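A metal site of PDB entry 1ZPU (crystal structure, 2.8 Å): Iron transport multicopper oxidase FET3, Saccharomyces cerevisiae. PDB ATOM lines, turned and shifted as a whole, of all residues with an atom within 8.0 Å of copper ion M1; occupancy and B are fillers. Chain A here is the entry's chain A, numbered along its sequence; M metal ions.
O of His 462 lies within hydrogen-bond range of N of His 395 (2.8 Å).
ND1 of His 397 lies within hydrogen-bond range of OD2 of Asp 73 (2.5 Å).
O of Phe 460 sits at hydrogen-bond distance from N of His 397 (3.1 Å).
Copper ion M1 is bound by NE2 of His 107, NE2 of His 397 and NE2 of His 462.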
ATOM      1  N   HIS A  60       5.200 -14.339   8.303  1.00  0.00           N
ATOM      2  CA  HIS A  60       5.047 -13.842   6.952  1.00  0.00           C
ATOM      3  C   HIS A  60       3.658 -14.194   6.464  1.00  0.00           C
ATOM      4  O   HIS A  60       3.178 -15.297   6.688  1.00  0.00           O
ATOM      5  CB  HIS A  60       6.090 -14.488   6.055  1.00  0.00           C
ATOM      6  CG  HIS A  60       5.815 -14.320   4.588  1.00  0.00           C
ATOM      7  ND1 HIS A  60       5.563 -13.099   4.013  1.00  0.00           N
ATOM      8  CD2 HIS A  60       5.782 -15.224   3.582  1.00  0.00           C
ATOM      9  CE1 HIS A  60       5.366 -13.249   2.722  1.00  0.00           C
ATOM     10  NE2 HIS A  60       5.498 -14.529   2.438  1.00  0.00           N
ATOM     11  N   HIS A  62       1.732 -14.977   3.344  1.00  0.00           N
ATOM     12  CA  HIS A  62       2.101 -15.429   2.023  1.00  0.00           C
ATOM     13  C   HIS A  62       1.140 -14.949   0.969  1.00  0.00           C
ATOM     14  O   HIS A  62      -0.041 -15.325   0.980  1.00  0.00           O
ATOM     15  CB  HIS A  62       2.139 -16.957   1.989  1.00  0.00           C
ATOM     16  CG  HIS A  62       2.669 -17.512   0.706  1.00  0.00           C
ATOM     17  ND1 HIS A  62       3.838 -18.233   0.637  1.00  0.00           N
ATOM     18  CD2 HIS A  62       2.189 -17.442  -0.559  1.00  0.00           C
ATOM     19  CE1 HIS A  62       4.058 -18.582  -0.619  1.00  0.00           C
ATOM     20  NE2 HIS A  62       3.074 -18.106  -1.361  1.00  0.00           N
ATOM     21  N   ASP A  73       6.145  -7.476   5.892  1.00  0.00           N
ATOM     22  CA  ASP A  73       6.231  -8.713   5.122  1.00  0.00           C
ATOM     23  C   ASP A  73       6.708  -9.912   5.935  1.00  0.00           C
ATOM     24  O   ASP A  73       6.415 -11.052   5.583  1.00  0.00           O
ATOM     25  CB  ASP A  73       7.150  -8.535   3.912  1.00  0.00           C
ATOM     26  CG  ASP A  73       6.931  -9.618   2.859  1.00  0.00           C
ATOM     27  OD1 ASP A  73       5.763  -9.960   2.606  1.00  0.00           O
ATOM     28  OD2 ASP A  73       7.931 -10.099   2.298  1.00  0.00           O
ATOM     29  N   GLY A  74       7.447  -9.642   7.004  1.00  0.00           N
ATOM     30  CA  GLY A  74       7.834 -10.672   7.965  1.00  0.00           C
ATOM     31  C   GLY A  74       8.995 -11.569   7.580  1.00  0.00           C
ATOM     32  O   GLY A  74       9.028 -12.723   7.975  1.00  0.00           O
ATOM     33  N   VAL A  75       9.954 -11.041   6.832  1.00  0.00           N
ATOM     34  CA  VAL A  75      11.150 -11.802   6.499  1.00  0.00           C
ATOM     35  C   VAL A  75      12.335 -11.177   7.214  1.00  0.00           C
ATOM     36  O   VAL A  75      12.735 -10.061   6.893  1.00  0.00           O
ATOM     37  CB  VAL A  75      11.420 -11.851   4.973  1.00  0.00           C
ATOM     38  CG1 VAL A  75      12.646 -12.683   4.696  1.00  0.00           C
ATOM     39  CG2 VAL A  75      10.229 -12.430   4.239  1.00  0.00           C
ATOM     40  N   LEU A  78      15.467  -9.052   5.728  1.00  0.00           N
ATOM     41  CA  LEU A  78      14.967  -8.405   4.519  1.00  0.00           C
ATOM     42  C   LEU A  78      14.110  -7.233   4.958  1.00  0.00           C
ATOM     43  O   LEU A  78      14.328  -6.074   4.566  1.00  0.00           O
ATOM     44  CB  LEU A  78      14.076  -9.356   3.729  1.00  0.00           C
ATOM     45  CG  LEU A  78      14.551 -10.444   2.760  1.00  0.00           C
ATOM     46  CD1 LEU A  78      14.339 -10.013   1.324  1.00  0.00           C
ATOM     47  CD2 LEU A  78      15.970 -10.896   3.013  1.00  0.00           C
ATOM     48  N   HIS A 105       2.766 -18.056   7.688  1.00  0.00           N
ATOM     49  CA  HIS A 105       3.690 -18.987   8.304  1.00  0.00           C
ATOM     50  C   HIS A 105       4.872 -18.243   8.887  1.00  0.00           C
ATOM     51  O   HIS A 105       5.174 -17.128   8.466  1.00  0.00           O
ATOM     52  CB  HIS A 105       4.190 -20.034   7.293  1.00  0.00           C
ATOM     53  CG  HIS A 105       4.849 -19.463   6.069  1.00  0.00           C
ATOM     54  ND1 HIS A 105       6.178 -19.094   6.040  1.00  0.00           N
ATOM     55  CD2 HIS A 105       4.362 -19.211   4.824  1.00  0.00           C
ATOM     56  CE1 HIS A 105       6.478 -18.631   4.842  1.00  0.00           C
ATOM     57  NE2 HIS A 105       5.400 -18.689   4.085  1.00  0.00           N
ATOM     58  N   SER A 106       5.525 -18.853   9.870  1.00  0.00           N
ATOM     59  CA  SER A 106       6.789 -18.347  10.376  1.00  0.00           C
ATOM     60  C   SER A 106       7.792 -18.311   9.244  1.00  0.00           C
ATOM     61  O   SER A 106       7.799 -19.200   8.393  1.00  0.00           O
ATOM     62  CB  SER A 106       7.303 -19.252  11.488  1.00  0.00           C
ATOM     63  OG  SER A 106       8.646 -18.959  11.823  1.00  0.00           O
ATOM     64  N   HIS A 107       8.630 -17.286   9.205  1.00  0.00           N
ATOM     65  CA  HIS A 107       9.689 -17.233   8.199  1.00  0.00           C
ATOM     66  C   HIS A 107      11.090 -17.395   8.813  1.00  0.00           C
ATOM     67  O   HIS A 107      12.087 -17.054   8.176  1.00  0.00           O
ATOM     68  CB  HIS A 107       9.594 -15.948   7.380  1.00  0.00           C
ATOM     69  CG  HIS A 107       9.886 -16.143   5.915  1.00  0.00           C
ATOM     70  ND1 HIS A 107      11.170 -16.256   5.429  1.00  0.00           N
ATOM     71  CD2 HIS A 107       9.060 -16.260   4.849  1.00  0.00           C
ATOM     72  CE1 HIS A 107      11.123 -16.423   4.125  1.00  0.00           C
ATOM     73  NE2 HIS A 107       9.855 -16.438   3.748  1.00  0.00           N
ATOM     74  N   TYR A 112       8.000 -23.119  10.645  1.00  0.00           N
ATOM     75  CA  TYR A 112       6.612 -23.438  10.236  1.00  0.00           C
ATOM     76  C   TYR A 112       6.274 -24.934  10.070  1.00  0.00           C
ATOM     77  O   TYR A 112       5.144 -25.331  10.329  1.00  0.00           O
ATOM     78  CB  TYR A 112       6.049 -22.572   9.100  1.00  0.00           C
ATOM     79  CG  TYR A 112       6.265 -23.037   7.673  1.00  0.00           C
ATOM     80  CD1 TYR A 112       5.460 -24.015   7.077  1.00  0.00           C
ATOM     81  CD2 TYR A 112       7.233 -22.424   6.887  1.00  0.00           C
ATOM     82  CE1 TYR A 112       5.649 -24.387   5.748  1.00  0.00           C
ATOM     83  CE2 TYR A 112       7.438 -22.776   5.575  1.00  0.00           C
ATOM     84  CZ  TYR A 112       6.652 -23.752   5.005  1.00  0.00           C
ATOM     85  OH  TYR A 112       6.916 -24.067   3.682  1.00  0.00           O
ATOM     86  N   HIS A 395       8.989 -19.051  -5.086  1.00  0.00           N
ATOM     87  CA  HIS A 395       7.965 -18.115  -4.707  1.00  0.00           C
ATOM     88  C   HIS A 395       8.548 -16.701  -4.666  1.00  0.00           C
ATOM     89  O   HIS A 395       9.719 -16.514  -4.290  1.00  0.00           O
ATOM     90  CB  HIS A 395       7.341 -18.539  -3.380  1.00  0.00           C
ATOM     91  CG  HIS A 395       6.609 -17.439  -2.684  1.00  0.00           C
ATOM     92  ND1 HIS A 395       5.473 -16.856  -3.194  1.00  0.00           N
ATOM     93  CD2 HIS A 395       6.872 -16.798  -1.528  1.00  0.00           C
ATOM     94  CE1 HIS A 395       5.062 -15.911  -2.381  1.00  0.00           C
ATOM     95  NE2 HIS A 395       5.896 -15.854  -1.359  1.00  0.00           N
ATOM     96  N   LEU A 396       7.712 -15.733  -5.067  1.00  0.00           N
ATOM     97  CA  LEU A 396       8.114 -14.336  -5.135  1.00  0.00           C
ATOM     98  C   LEU A 396       7.256 -13.485  -4.233  1.00  0.00           C
ATOM     99  O   LEU A 396       6.034 -13.430  -4.405  1.00  0.00           O
ATOM    100  CB  LEU A 396       8.025 -13.832  -6.571  1.00  0.00           C
ATOM    101  CG  LEU A 396       8.325 -12.348  -6.868  1.00  0.00           C
ATOM    102  CD1 LEU A 396       9.796 -11.963  -6.617  1.00  0.00           C
ATOM    103  CD2 LEU A 396       7.905 -12.010  -8.296  1.00  0.00           C
ATOM    104  N   HIS A 397       7.877 -12.799  -3.278  1.00  0.00           N
ATOM    105  CA  HIS A 397       7.161 -11.896  -2.378  1.00  0.00           C
ATOM    106  C   HIS A 397       6.725 -10.634  -3.132  1.00  0.00           C
ATOM    107  O   HIS A 397       7.371 -10.247  -4.109  1.00  0.00           O
ATOM    108  CB  HIS A 397       8.043 -11.478  -1.212  1.00  0.00           C
ATOM    109  CG  HIS A 397       8.247 -12.557  -0.201  1.00  0.00           C
ATOM    110  ND1 HIS A 397       8.018 -12.369   1.147  1.00  0.00           N
ATOM    111  CD2 HIS A 397       8.694 -13.833  -0.324  1.00  0.00           C
ATOM    112  CE1 HIS A 397       8.306 -13.476   1.799  1.00  0.00           C
ATOM    113  NE2 HIS A 397       8.709 -14.389   0.934  1.00  0.00           N
ATOM    114  N   TRP A 459      11.819  -7.561  -1.587  1.00  0.00           N
ATOM    115  CA  TRP A 459      11.110  -8.808  -1.838  1.00  0.00           C
ATOM    116  C   TRP A 459      12.023 -10.028  -2.018  1.00  0.00           C
ATOM    117  O   TRP A 459      12.925 -10.007  -2.839  1.00  0.00           O
ATOM    118  CB  TRP A 459      10.195  -8.676  -3.064  1.00  0.00           C
ATOM    119  CG  TRP A 459       9.298  -7.471  -3.083  1.00  0.00           C
ATOM    120  CD1 TRP A 459       9.289  -6.499  -4.026  1.00  0.00           C
ATOM    121  CD2 TRP A 459       8.283  -7.116  -2.137  1.00  0.00           C
ATOM    122  NE1 TRP A 459       8.344  -5.552  -3.730  1.00  0.00           N
ATOM    123  CE2 TRP A 459       7.703  -5.910  -2.578  1.00  0.00           C
ATOM    124  CE3 TRP A 459       7.809  -7.687  -0.950  1.00  0.00           C
ATOM    125  CZ2 TRP A 459       6.683  -5.279  -1.887  1.00  0.00           C
ATOM    126  CZ3 TRP A 459       6.784  -7.060  -0.266  1.00  0.00           C
ATOM    127  CH2 TRP A 459       6.231  -5.871  -0.734  1.00  0.00           C
ATOM    128  N   PHE A 460      11.735 -11.088  -1.261  1.00  0.00           N
ATOM    129  CA  PHE A 460      12.497 -12.320  -1.286  1.00  0.00           C
ATOM    130  C   PHE A 460      12.054 -13.175  -2.475  1.00  0.00           C
ATOM    131  O   PHE A 460      10.852 -13.363  -2.687  1.00  0.00           O
ATOM    132  CB  PHE A 460      12.306 -13.086   0.041  1.00  0.00           C
ATOM    133  CG  PHE A 460      13.518 -13.861   0.509  1.00  0.00           C
ATOM    134  CD1 PHE A 460      14.731 -13.800  -0.166  1.00  0.00           C
ATOM    135  CD2 PHE A 460      13.440 -14.636   1.667  1.00  0.00           C
ATOM    136  CE1 PHE A 460      15.848 -14.526   0.297  1.00  0.00           C
ATOM    137  CE2 PHE A 460      14.560 -15.353   2.150  1.00  0.00           C
ATOM    138  CZ  PHE A 460      15.756 -15.304   1.454  1.00  0.00           C
ATOM    139  N   PHE A 461      13.010 -13.654  -3.252  1.00  0.00           N
ATOM    140  CA  PHE A 461      12.729 -14.655  -4.271  1.00  0.00           C
ATOM    141  C   PHE A 461      13.496 -15.936  -3.968  1.00  0.00           C
ATOM    142  O   PHE A 461      14.727 -15.947  -4.034  1.00  0.00           O
ATOM    143  CB  PHE A 461      13.063 -14.150  -5.671  1.00  0.00           C
ATOM    144  CG  PHE A 461      12.804 -15.160  -6.744  1.00  0.00           C
ATOM    145  CD1 PHE A 461      11.513 -15.403  -7.189  1.00  0.00           C
ATOM    146  CD2 PHE A 461      13.865 -15.897  -7.287  1.00  0.00           C
ATOM    147  CE1 PHE A 461      11.276 -16.342  -8.178  1.00  0.00           C
ATOM    148  CE2 PHE A 461      13.623 -16.849  -8.280  1.00  0.00           C
ATOM    149  CZ  PHE A 461      12.327 -17.069  -8.719  1.00  0.00           C
ATOM    150  N   HIS A 462      12.773 -17.002  -3.623  1.00  0.00           N
ATOM    151  CA  HIS A 462      13.417 -18.217  -3.144  1.00  0.00           C
ATOM    152  C   HIS A 462      12.598 -19.457  -3.393  1.00  0.00           C
ATOM    153  O   HIS A 462      11.401 -19.394  -3.687  1.00  0.00           O
ATOM    154  CB  HIS A 462      13.659 -18.113  -1.642  1.00  0.00           C
ATOM    155  CG  HIS A 462      12.398 -18.061  -0.836  1.00  0.00           C
ATOM    156  ND1 HIS A 462      11.781 -19.194  -0.346  1.00  0.00           N
ATOM    157  CD2 HIS A 462      11.628 -17.020  -0.453  1.00  0.00           C
ATOM    158  CE1 HIS A 462      10.690 -18.852   0.307  1.00  0.00           C
ATOM    159  NE2 HIS A 462      10.564 -17.539   0.249  1.00  0.00           N
ATOM    160  N   CYS A 463      13.250 -20.597  -3.211  1.00  0.00           N
ATOM    161  CA  CYS A 463      12.582 -21.876  -3.158  1.00  0.00           C
ATOM    162  C   CYS A 463      11.846 -22.018  -1.823  1.00  0.00           C
ATOM    163  O   CYS A 463      12.386 -21.726  -0.759  1.00  0.00           O
ATOM    164  CB  CYS A 463      13.591 -23.001  -3.328  1.00  0.00           C
ATOM    165  SG  CYS A 463      12.830 -24.611  -3.384  1.00  0.00           S
ATOM    166  N   HIS A 464      10.609 -22.478  -1.889  1.00  0.00           N
ATOM    167  CA  HIS A 464       9.784 -22.602  -0.714  1.00  0.00           C
ATOM    168  C   HIS A 464       9.943 -23.947   0.016  1.00  0.00           C
ATOM    169  O   HIS A 464       9.246 -24.215   0.984  1.00  0.00           O
ATOM    170  CB  HIS A 464       8.330 -22.341  -1.046  1.00  0.00           C
ATOM    171  CG  HIS A 464       7.585 -21.656   0.049  1.00  0.00           C
ATOM    172  ND1 HIS A 464       7.236 -22.303   1.218  1.00  0.00           N
ATOM    173  CD2 HIS A 464       7.137 -20.380   0.172  1.00  0.00           C
ATOM    174  CE1 HIS A 464       6.612 -21.450   2.014  1.00  0.00           C
ATOM    175  NE2 HIS A 464       6.533 -20.277   1.396  1.00  0.00           N
ATOM    176  N   GLU A 466      11.644 -25.721   2.612  1.00  0.00           N
ATOM    177  CA  GLU A 466      12.327 -25.203   3.774  1.00  0.00           C
ATOM    178  C   GLU A 466      13.796 -25.606   3.864  1.00  0.00           C
ATOM    179  O   GLU A 466      14.654 -24.798   4.243  1.00  0.00           O
ATOM    180  CB  GLU A 466      11.556 -25.609   5.014  1.00  0.00           C
ATOM    181  CG  GLU A 466      10.411 -24.639   5.305  1.00  0.00           C
ATOM    182  CD  GLU A 466      10.911 -23.311   5.903  1.00  0.00           C
ATOM    183  OE1 GLU A 466      11.393 -23.342   7.076  1.00  0.00           O
ATOM    184  OE2 GLU A 466      10.836 -22.270   5.199  1.00  0.00           O
ATOM    185  N   LEU A 469      15.788 -23.486   1.350  1.00  0.00           N
ATOM    186  CA  LEU A 469      15.939 -22.137   1.857  1.00  0.00           C
ATOM    187  C   LEU A 469      17.017 -22.105   2.947  1.00  0.00           C
ATOM    188  O   LEU A 469      17.799 -21.152   3.018  1.00  0.00           O
ATOM    189  CB  LEU A 469      14.613 -21.639   2.393  1.00  0.00           C
ATOM    190  CG  LEU A 469      14.524 -20.198   2.891  1.00  0.00           C
ATOM    191  CD1 LEU A 469      14.858 -19.164   1.792  1.00  0.00           C
ATOM    192  CD2 LEU A 469      13.139 -19.970   3.508  1.00  0.00           C
HETATM  193 CU    CU M   1       9.565 -16.188   1.693  1.00  0.00          CU
HETATM  194 CU    CU M   2       5.356 -14.959   0.405  1.00  0.00          CU
HETATM  195 CU    CU M   3       5.118 -18.675   2.039  1.00  0.00          CU
